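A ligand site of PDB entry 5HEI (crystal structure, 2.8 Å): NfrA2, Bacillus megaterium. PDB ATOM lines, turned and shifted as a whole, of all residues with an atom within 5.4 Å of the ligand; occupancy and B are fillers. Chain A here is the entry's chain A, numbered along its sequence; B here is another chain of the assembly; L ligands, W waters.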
ATOM      1  N   HIS A  11      20.540   0.572 -26.445  1.00  0.00           N
ATOM      2  CA  HIS A  11      19.540   0.835 -25.419  1.00  0.00           C
ATOM      3  C   HIS A  11      18.139   1.114 -25.960  1.00  0.00           C
ATOM      4  O   HIS A  11      17.943   1.932 -26.858  1.00  0.00           O
ATOM      5  CB  HIS A  11      19.980   1.934 -24.434  1.00  0.00           C
ATOM      6  CG  HIS A  11      18.899   2.319 -23.464  1.00  0.00           C
ATOM      7  ND1 HIS A  11      18.544   1.488 -22.400  1.00  0.00           N
ATOM      8  CD2 HIS A  11      18.085   3.399 -23.453  1.00  0.00           C
ATOM      9  CE1 HIS A  11      17.550   2.109 -21.786  1.00  0.00           C
ATOM     10  NE2 HIS A  11      17.243   3.258 -22.385  1.00  0.00           N
ATOM     11  N   ARG A  12      17.183   0.358 -25.405  1.00  0.00           N
ATOM     12  CA  ARG A  12      15.756   0.459 -25.678  1.00  0.00           C
ATOM     13  C   ARG A  12      15.029   0.154 -24.366  1.00  0.00           C
ATOM     14  O   ARG A  12      15.288  -0.865 -23.736  1.00  0.00           O
ATOM     15  CB  ARG A  12      15.299  -0.443 -26.868  1.00  0.00           C
ATOM     16  CG  ARG A  12      15.647  -1.943 -26.778  1.00  0.00           C
ATOM     17  CD  ARG A  12      16.547  -2.435 -27.911  1.00  0.00           C
ATOM     18  NE  ARG A  12      15.874  -2.477 -29.209  1.00  0.00           N
ATOM     19  CZ  ARG A  12      16.202  -3.291 -30.211  1.00  0.00           C
ATOM     20  NH1 ARG A  12      17.199  -4.166 -30.071  1.00  0.00           N
ATOM     21  NH2 ARG A  12      15.535  -3.250 -31.363  1.00  0.00           N
ATOM     22  N   SER A  13      14.210   1.113 -23.903  1.00  0.00           N
ATOM     23  CA  SER A  13      13.432   0.932 -22.679  1.00  0.00           C
ATOM     24  C   SER A  13      12.175   0.163 -23.040  1.00  0.00           C
ATOM     25  O   SER A  13      11.566   0.443 -24.083  1.00  0.00           O
ATOM     26  CB  SER A  13      13.087   2.281 -22.049  1.00  0.00           C
ATOM     27  OG  SER A  13      14.160   2.807 -21.287  1.00  0.00           O
ATOM     28  N   ARG A  15       8.268  -1.533 -21.845  1.00  0.00           N
ATOM     29  CA  ARG A  15       7.081  -1.413 -20.989  1.00  0.00           C
ATOM     30  C   ARG A  15       6.230  -2.695 -21.035  1.00  0.00           C
ATOM     31  O   ARG A  15       5.238  -2.809 -20.310  1.00  0.00           O
ATOM     32  CB  ARG A  15       6.266  -0.155 -21.350  1.00  0.00           C
ATOM     33  CG  ARG A  15       6.980   1.143 -20.939  1.00  0.00           C
ATOM     34  CD  ARG A  15       6.401   2.361 -21.627  1.00  0.00           C
ATOM     35  NE  ARG A  15       7.411   3.421 -21.743  1.00  0.00           N
ATOM     36  CZ  ARG A  15       8.258   3.541 -22.761  1.00  0.00           C
ATOM     37  NH1 ARG A  15       8.220   2.688 -23.776  1.00  0.00           N
ATOM     38  NH2 ARG A  15       9.156   4.522 -22.769  1.00  0.00           N
ATOM     39  N   ALA A  64       2.472   6.874  -9.399  1.00  0.00           N
ATOM     40  CA  ALA A  64       3.377   7.290 -10.479  1.00  0.00           C
ATOM     41  C   ALA A  64       2.601   7.688 -11.748  1.00  0.00           C
ATOM     42  O   ALA A  64       3.204   8.079 -12.752  1.00  0.00           O
ATOM     43  CB  ALA A  64       4.378   6.180 -10.783  1.00  0.00           C
ATOM     44  N   GLN A  67       0.821   3.695 -14.253  1.00  0.00           N
ATOM     45  CA  GLN A  67       1.667   3.074 -15.280  1.00  0.00           C
ATOM     46  C   GLN A  67       1.606   1.562 -15.170  1.00  0.00           C
ATOM     47  O   GLN A  67       2.132   0.986 -14.214  1.00  0.00           O
ATOM     48  CB  GLN A  67       3.108   3.602 -15.220  1.00  0.00           C
ATOM     49  CG  GLN A  67       3.238   5.076 -15.578  1.00  0.00           C
ATOM     50  CD  GLN A  67       4.637   5.596 -15.351  1.00  0.00           C
ATOM     51  OE1 GLN A  67       5.590   5.216 -16.030  1.00  0.00           O
ATOM     52  NE2 GLN A  67       4.780   6.512 -14.396  1.00  0.00           N
ATOM     53  N   TRP A  69       3.089  -0.857 -16.640  1.00  0.00           N
ATOM     54  CA  TRP A  69       4.389  -1.526 -16.630  1.00  0.00           C
ATOM     55  C   TRP A  69       4.991  -1.745 -15.249  1.00  0.00           C
ATOM     56  O   TRP A  69       5.777  -2.675 -15.083  1.00  0.00           O
ATOM     57  CB  TRP A  69       5.386  -0.885 -17.608  1.00  0.00           C
ATOM     58  CG  TRP A  69       5.338   0.610 -17.707  1.00  0.00           C
ATOM     59  CD1 TRP A  69       6.199   1.498 -17.121  1.00  0.00           C
ATOM     60  CD2 TRP A  69       4.441   1.394 -18.504  1.00  0.00           C
ATOM     61  NE1 TRP A  69       5.871   2.783 -17.478  1.00  0.00           N
ATOM     62  CE2 TRP A  69       4.804   2.745 -18.335  1.00  0.00           C
ATOM     63  CE3 TRP A  69       3.361   1.087 -19.353  1.00  0.00           C
ATOM     64  CZ2 TRP A  69       4.102   3.795 -18.961  1.00  0.00           C
ATOM     65  CZ3 TRP A  69       2.678   2.111 -19.971  1.00  0.00           C
ATOM     66  CH2 TRP A  69       3.056   3.452 -19.779  1.00  0.00           C
ATOM     67  N   LEU A 117      21.434   4.708 -11.120  1.00  0.00           N
ATOM     68  CA  LEU A 117      20.355   4.204 -11.978  1.00  0.00           C
ATOM     69  C   LEU A 117      20.935   3.672 -13.293  1.00  0.00           C
ATOM     70  O   LEU A 117      20.593   2.561 -13.702  1.00  0.00           O
ATOM     71  CB  LEU A 117      19.337   5.307 -12.229  1.00  0.00           C
ATOM     72  CG  LEU A 117      17.977   4.888 -12.756  1.00  0.00           C
ATOM     73  CD1 LEU A 117      16.874   5.617 -12.027  1.00  0.00           C
ATOM     74  CD2 LEU A 117      17.864   5.165 -14.247  1.00  0.00           C
ATOM     75  N   VAL A 132      13.182   0.458 -17.463  1.00  0.00           N
ATOM     76  CA  VAL A 132      12.512   1.737 -17.726  1.00  0.00           C
ATOM     77  C   VAL A 132      12.491   2.553 -16.425  1.00  0.00           C
ATOM     78  O   VAL A 132      11.915   2.087 -15.434  1.00  0.00           O
ATOM     79  CB  VAL A 132      11.146   1.670 -18.485  1.00  0.00           C
ATOM     80  CG1 VAL A 132      10.045   0.985 -17.659  1.00  0.00           C
ATOM     81  CG2 VAL A 132      10.698   3.055 -18.944  1.00  0.00           C
ATOM     82  N   PRO A 133      13.191   3.710 -16.364  1.00  0.00           N
ATOM     83  CA  PRO A 133      13.164   4.516 -15.128  1.00  0.00           C
ATOM     84  C   PRO A 133      11.779   5.142 -14.933  1.00  0.00           C
ATOM     85  O   PRO A 133      11.073   5.363 -15.910  1.00  0.00           O
ATOM     86  CB  PRO A 133      14.230   5.582 -15.371  1.00  0.00           C
ATOM     87  CG  PRO A 133      14.950   5.162 -16.629  1.00  0.00           C
ATOM     88  CD  PRO A 133      13.956   4.394 -17.417  1.00  0.00           C
ATOM     89  N   ILE A 134      11.369   5.372 -13.674  1.00  0.00           N
ATOM     90  CA  ILE A 134      10.075   5.979 -13.385  1.00  0.00           C
ATOM     91  C   ILE A 134      10.260   7.280 -12.596  1.00  0.00           C
ATOM     92  O   ILE A 134      10.209   7.272 -11.364  1.00  0.00           O
ATOM     93  CB  ILE A 134       9.027   4.999 -12.758  1.00  0.00           C
ATOM     94  CG1 ILE A 134       8.919   3.652 -13.518  1.00  0.00           C
ATOM     95  CG2 ILE A 134       7.650   5.667 -12.564  1.00  0.00           C
ATOM     96  CD1 ILE A 134       8.308   3.645 -14.997  1.00  0.00           C
ATOM     97  N   GLY A 135      10.455   8.370 -13.330  1.00  0.00           N
ATOM     98  CA  GLY A 135      10.605   9.727 -12.783  1.00  0.00           C
ATOM     99  C   GLY A 135       9.304  10.239 -12.193  1.00  0.00           C
ATOM    100  O   GLY A 135       9.305  11.238 -11.460  1.00  0.00           O
ATOM    101  N   GLY A 136       8.213   9.510 -12.487  1.00  0.00           N
ATOM    102  CA  GLY A 136       6.857   9.750 -12.008  1.00  0.00           C
ATOM    103  C   GLY A 136       6.652   9.565 -10.519  1.00  0.00           C
ATOM    104  O   GLY A 136       5.591   9.889  -9.999  1.00  0.00           O
ATOM    105  N   ARG A 138       7.788  11.341  -8.317  1.00  0.00           N
ATOM    106  CA  ARG A 138       7.692  12.698  -7.813  1.00  0.00           C
ATOM    107  C   ARG A 138       6.314  13.336  -8.097  1.00  0.00           C
ATOM    108  O   ARG A 138       6.123  14.529  -7.844  1.00  0.00           O
ATOM    109  CB  ARG A 138       8.834  13.572  -8.373  1.00  0.00           C
ATOM    110  CG  ARG A 138      10.193  13.290  -7.733  1.00  0.00           C
ATOM    111  CD  ARG A 138      11.324  13.882  -8.545  1.00  0.00           C
ATOM    112  NE  ARG A 138      11.539  13.138  -9.789  1.00  0.00           N
ATOM    113  CZ  ARG A 138      12.091  13.652 -10.882  1.00  0.00           C
ATOM    114  NH1 ARG A 138      12.479  14.914 -10.908  1.00  0.00           N
ATOM    115  NH2 ARG A 138      12.253  12.892 -11.955  1.00  0.00           N
ATOM    116  N   SER A 158      14.090   8.734  -8.555  1.00  0.00           N
ATOM    117  CA  SER A 158      13.495   8.021  -9.684  1.00  0.00           C
ATOM    118  C   SER A 158      13.403   6.529  -9.402  1.00  0.00           C
ATOM    119  O   SER A 158      14.220   5.964  -8.671  1.00  0.00           O
ATOM    120  CB  SER A 158      14.305   8.258 -10.963  1.00  0.00           C
ATOM    121  OG  SER A 158      13.749   7.603 -12.097  1.00  0.00           O
ATOM    122  N   ALA A 170      11.783  -0.901 -30.168  1.00  0.00           N
ATOM    123  CA  ALA A 170      12.606  -0.170 -31.143  1.00  0.00           C
ATOM    124  C   ALA A 170      13.340   1.009 -30.503  1.00  0.00           C
ATOM    125  O   ALA A 170      12.763   1.716 -29.675  1.00  0.00           O
ATOM    126  CB  ALA A 170      11.743   0.315 -32.300  1.00  0.00           C
ATOM    127  N   LYS A 171      14.617   1.228 -30.924  1.00  0.00           N
ATOM    128  CA  LYS A 171      15.477   2.327 -30.472  1.00  0.00           C
ATOM    129  C   LYS A 171      14.871   3.682 -30.886  1.00  0.00           C
ATOM    130  O   LYS A 171      14.571   3.902 -32.066  1.00  0.00           O
ATOM    131  CB  LYS A 171      16.872   2.173 -31.106  1.00  0.00           C
ATOM    132  CG  LYS A 171      17.976   1.671 -30.173  1.00  0.00           C
ATOM    133  CD  LYS A 171      18.975   0.760 -30.884  1.00  0.00           C
ATOM    134  CE  LYS A 171      19.845   1.448 -31.909  1.00  0.00           C
ATOM    135  NZ  LYS A 171      20.272   0.497 -32.986  1.00  0.00           N
ATOM    136  N   LYS A 172      14.664   4.581 -29.904  1.00  0.00           N
ATOM    137  CA  LYS A 172      14.143   5.932 -30.161  1.00  0.00           C
ATOM    138  C   LYS A 172      15.320   6.786 -30.660  1.00  0.00           C
ATOM    139  O   LYS A 172      16.348   6.838 -29.984  1.00  0.00           O
ATOM    140  CB  LYS A 172      13.577   6.570 -28.862  1.00  0.00           C
ATOM    141  CG  LYS A 172      12.077   6.447 -28.662  1.00  0.00           C
ATOM    142  CD  LYS A 172      11.670   7.197 -27.404  1.00  0.00           C
ATOM    143  CE  LYS A 172      10.261   6.909 -26.958  1.00  0.00           C
ATOM    144  NZ  LYS A 172       9.291   7.887 -27.529  1.00  0.00           N
ATOM    145  N   ARG A 174      17.972   9.756 -31.288  1.00  0.00           N
ATOM    146  CA  ARG A 174      18.453  10.834 -30.403  1.00  0.00           C
ATOM    147  C   ARG A 174      18.864  12.066 -31.213  1.00  0.00           C
ATOM    148  O   ARG A 174      19.065  11.977 -32.424  1.00  0.00           O
ATOM    149  CB  ARG A 174      19.610  10.350 -29.511  1.00  0.00           C
ATOM    150  CG  ARG A 174      19.277   9.183 -28.561  1.00  0.00           C
ATOM    151  CD  ARG A 174      18.323   9.552 -27.435  1.00  0.00           C
ATOM    152  NE  ARG A 174      18.322   8.545 -26.372  1.00  0.00           N
ATOM    153  CZ  ARG A 174      17.508   7.505 -26.315  1.00  0.00           C
ATOM    154  NH1 ARG A 174      16.590   7.314 -27.259  1.00  0.00           N
ATOM    155  NH2 ARG A 174      17.589   6.640 -25.307  1.00  0.00           N
ATOM    156  N   SER B  36      23.079   7.702 -26.106  1.00  0.00           N
ATOM    157  CA  SER B  36      22.331   6.445 -26.161  1.00  0.00           C
ATOM    158  C   SER B  36      21.591   6.101 -24.860  1.00  0.00           C
ATOM    159  O   SER B  36      20.674   5.294 -24.883  1.00  0.00           O
ATOM    160  CB  SER B  36      23.252   5.302 -26.557  1.00  0.00           C
ATOM    161  OG  SER B  36      23.689   5.440 -27.902  1.00  0.00           O
ATOM    162  N   ALA B  38      19.125   6.703 -21.399  1.00  0.00           N
ATOM    163  CA  ALA B  38      17.762   7.189 -21.203  1.00  0.00           C
ATOM    164  C   ALA B  38      17.713   8.629 -20.690  1.00  0.00           C
ATOM    165  O   ALA B  38      18.620   9.062 -19.973  1.00  0.00           O
ATOM    166  CB  ALA B  38      17.023   6.272 -20.237  1.00  0.00           C
ATOM    167  N   SER B  39      16.660   9.376 -21.049  1.00  0.00           N
ATOM    168  CA  SER B  39      16.421  10.766 -20.617  1.00  0.00           C
ATOM    169  C   SER B  39      14.943  10.976 -20.335  1.00  0.00           C
ATOM    170  O   SER B  39      14.099  10.470 -21.086  1.00  0.00           O
ATOM    171  CB  SER B  39      16.926  11.758 -21.655  1.00  0.00           C
ATOM    172  OG  SER B  39      16.257  11.632 -22.897  1.00  0.00           O
ATOM    173  N   SER B  40      14.613  11.707 -19.244  1.00  0.00           N
ATOM    174  CA  SER B  40      13.235  11.998 -18.830  1.00  0.00           C
ATOM    175  C   SER B  40      12.444  12.584 -19.995  1.00  0.00           C
ATOM    176  O   SER B  40      12.884  13.577 -20.591  1.00  0.00           O
ATOM    177  CB  SER B  40      13.220  12.938 -17.632  1.00  0.00           C
ATOM    178  OG  SER B  40      11.922  13.062 -17.082  1.00  0.00           O
ATOM    179  N   ILE B  41      11.324  11.920 -20.373  1.00  0.00           N
ATOM    180  CA  ILE B  41      10.409  12.256 -21.478  1.00  0.00           C
ATOM    181  C   ILE B  41      11.074  12.419 -22.879  1.00  0.00           C
ATOM    182  O   ILE B  41      10.494  13.043 -23.774  1.00  0.00           O
ATOM    183  CB  ILE B  41       9.358  13.368 -21.109  1.00  0.00           C
ATOM    184  CG1 ILE B  41       9.971  14.775 -20.929  1.00  0.00           C
ATOM    185  CG2 ILE B  41       8.502  12.959 -19.903  1.00  0.00           C
ATOM    186  CD1 ILE B  41       9.726  15.739 -22.044  1.00  0.00           C
ATOM    187  N   ASN B  42      12.280  11.817 -23.058  1.00  0.00           N
ATOM    188  CA  ASN B  42      13.142  11.894 -24.243  1.00  0.00           C
ATOM    189  C   ASN B  42      13.495  13.352 -24.597  1.00  0.00           C
ATOM    190  O   ASN B  42      13.719  13.698 -25.760  1.00  0.00           O
ATOM    191  CB  ASN B  42      12.589  11.109 -25.459  1.00  0.00           C
ATOM    192  CG  ASN B  42      13.614  10.848 -26.532  1.00  0.00           C
ATOM    193  OD1 ASN B  42      14.558  10.067 -26.367  1.00  0.00           O
ATOM    194  ND2 ASN B  42      13.505  11.549 -27.650  1.00  0.00           N
ATOM    195  N   THR B 111      19.544  14.699 -12.520  1.00  0.00           N
ATOM    196  CA  THR B 111      19.419  13.240 -12.618  1.00  0.00           C
ATOM    197  C   THR B 111      19.851  12.773 -14.002  1.00  0.00           C
ATOM    198  O   THR B 111      20.632  11.827 -14.101  1.00  0.00           O
ATOM    199  CB  THR B 111      18.008  12.765 -12.225  1.00  0.00           C
ATOM    200  OG1 THR B 111      17.639  13.336 -10.966  1.00  0.00           O
ATOM    201  CG2 THR B 111      17.895  11.265 -12.139  1.00  0.00           C
ATOM    202  N   ASP B 112      19.369  13.442 -15.085  1.00  0.00           N
ATOM    203  CA  ASP B 112      19.705  13.121 -16.471  1.00  0.00           C
ATOM    204  C   ASP B 112      21.203  13.307 -16.781  1.00  0.00           C
ATOM    205  O   ASP B 112      21.757  12.527 -17.559  1.00  0.00           O
ATOM    206  CB  ASP B 112      18.819  13.903 -17.462  1.00  0.00           C
ATOM    207  CG  ASP B 112      17.405  13.364 -17.692  1.00  0.00           C
ATOM    208  OD1 ASP B 112      16.837  12.738 -16.749  1.00  0.00           O
ATOM    209  OD2 ASP B 112      16.842  13.601 -18.784  1.00  0.00           O
ATOM    210  N   ILE B 115      23.149  10.408 -15.311  1.00  0.00           N
ATOM    211  CA  ILE B 115      22.934   9.258 -16.203  1.00  0.00           C
ATOM    212  C   ILE B 115      23.972   9.310 -17.358  1.00  0.00           C
ATOM    213  O   ILE B 115      24.711   8.344 -17.563  1.00  0.00           O
ATOM    214  CB  ILE B 115      21.456   9.215 -16.713  1.00  0.00           C
ATOM    215  CG1 ILE B 115      20.494   8.717 -15.622  1.00  0.00           C
ATOM    216  CG2 ILE B 115      21.298   8.358 -17.971  1.00  0.00           C
ATOM    217  CD1 ILE B 115      19.120   9.282 -15.660  1.00  0.00           C
HETATM  218  N1  LIG L   1       9.220   6.320 -18.948  1.00  0.00           N
HETATM  219  C1  LIG L   1       7.944   6.088 -18.520  1.00  0.00           C
HETATM  220  O1  LIG L   1       7.192   5.299 -19.114  1.00  0.00           O
HETATM  221  N2  LIG L   1       7.453   6.726 -17.379  1.00  0.00           N
HETATM  222  C2  LIG L   1       8.172   7.621 -16.586  1.00  0.00           C
HETATM  223  O2  LIG L   1       7.626   8.156 -15.617  1.00  0.00           O
HETATM  224  C3  LIG L   1       9.550   7.846 -17.038  1.00  0.00           C
HETATM  225  N3  LIG L   1      10.337   8.564 -16.278  1.00  0.00           N
HETATM  226  C4  LIG L   1      11.681   8.651 -16.633  1.00  0.00           C
HETATM  227  C5  LIG L   1      12.566   9.299 -15.754  1.00  0.00           C
HETATM  228  C6  LIG L   1      13.931   9.334 -15.998  1.00  0.00           C
HETATM  229  C7  LIG L   1      14.841   9.994 -14.977  1.00  0.00           C
HETATM  230  C8  LIG L   1      14.444   8.739 -17.168  1.00  0.00           C
HETATM  231  C9  LIG L   1      15.909   8.755 -17.488  1.00  0.00           C
HETATM  232  C10 LIG L   1      13.562   8.115 -18.046  1.00  0.00           C
HETATM  233  C11 LIG L   1      12.196   8.044 -17.797  1.00  0.00           C
HETATM  234  N4  LIG L   1      11.301   7.301 -18.607  1.00  0.00           N
HETATM  235  C12 LIG L   1       9.992   7.150 -18.246  1.00  0.00           C
HETATM  236  C13 LIG L   1      11.774   6.682 -19.861  1.00  0.00           C
HETATM  237  C14 LIG L   1      11.860   7.660 -21.035  1.00  0.00           C
HETATM  238  O3  LIG L   1      10.570   7.924 -21.589  1.00  0.00           O
HETATM  239  C15 LIG L   1      12.785   7.084 -22.106  1.00  0.00           C
HETATM  240  O4  LIG L   1      14.044   6.781 -21.511  1.00  0.00           O
HETATM  241  C16 LIG L   1      13.003   7.984 -23.326  1.00  0.00           C
HETATM  242  O5  LIG L   1      11.803   8.060 -24.097  1.00  0.00           O
HETATM  243  C17 LIG L   1      14.178   7.555 -24.191  1.00  0.00           C
HETATM  244  O6  LIG L   1      13.816   6.338 -24.877  1.00  0.00           O
HETATM  245  P1  LIG L   1      14.600   4.926 -24.762  1.00  0.00           P
HETATM  246  O7  LIG L   1      15.679   4.826 -25.787  1.00  0.00           O
HETATM  247  O8  LIG L   1      13.529   3.855 -24.964  1.00  0.00           O
HETATM  248  O9  LIG L   1      15.117   4.810 -23.328  1.00  0.00           O
HETATM  249  O   HOH W   1       7.219   8.244 -21.727  1.00  0.00           O
HETATM  250  O   HOH W   2       8.632   9.617 -19.589  1.00  0.00           O
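The guanidinium group (NE) of Arg 15 lies within hydrogen-bond range of an oxygen (O1) of the ligand (3.2 Å). NE1 of Trp 69 lies within hydrogen-bond range of O1 of the ligand (3.3 Å). The backbone NH (N) of Ser 13 is in hydrogen-bond range of an oxygen (O8) of the ligand. O7 of the ligand lies within salt-bridge range of NH2 of Arg 174 (2.7 Å). The side-chain hydroxyl (OG) of Ser 13 sits at hydrogen-bond distance from an oxygen (O9) of the ligand, at 3.0 Å. An oxygen (O9) of the ligand is in hydrogen-bond range of a ring nitrogen (NE2) of His 11, at 2.8 Å. N of Gly 136 lies within hydrogen-bond range of O2 of the ligand, at 3.5 Å. A nitrogen (N2) of the ligand sits at hydrogen-bond distance from the side-chain amide oxygen of Gln 67 (2.8 Å). N of Gly 135 sits at hydrogen-bond distance from N3 of the ligand, 3.0 Å away.
The backbone carbonyl oxygen (O) of Pro 133 lies close to a nitrogen (N3) of the ligand, 3.3 Å away. Merely in contact with the ligand: Val 132 (3.6 Å), Ile 134 (3.9 Å), Ser 158 (3.9 Å), Lys 172 (3.4 Å), Ala 38 of chain B (3.3 Å), Ser 39 of chain B (3.5 Å), Ser 40 of chain B (3.6 Å), Asn 42 of chain B (3.3 Å), Asp 112 of chain B (3.8 Å) and Ile 115 of chain B (3.7 Å). 19 residues have an atom within 4 Å of the ligand: His 11, Ser 13, Arg 15, Gln 67, Trp 69, Val 132, Pro 133, Ile 134, Gly 135, Gly 136, Ser 158, Lys 172, Arg 174, Ala 38 of chain B, Ser 39 of chain B, Ser 40 of chain B, Asn 42 of chain B, Asp 112 of chain B and Ile 115 of chain B.
The backbone NH of Ser 40 of chain B sits at hydrogen-bond distance from the side-chain carboxylate of Asp 112 of chain B (3.0 Å). The side-chain hydroxyl of Ser 13 lies within hydrogen-bond range of a ring nitrogen (NE2) of His 11, 3.3 Å away. The guanidinium group (NH2) of Arg 174 is in hydrogen-bond range of the backbone carbonyl oxygen (O) of Ser 36 of chain B (3.4 Å). The guanidinium group (NH1) of Arg 174 lies within hydrogen-bond range of the backbone carbonyl oxygen (O) of Lys 172, at 2.8 Å. NE2 of Gln 67 is in hydrogen-bond range of O of Ala 64, at 2.8 Å. OE1 of Gln 67 is in hydrogen-bond range of NE1 of Trp 69 (2.8 Å). NE of Arg 138 is in hydrogen-bond range of O of Gly 135 (3.4 Å).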
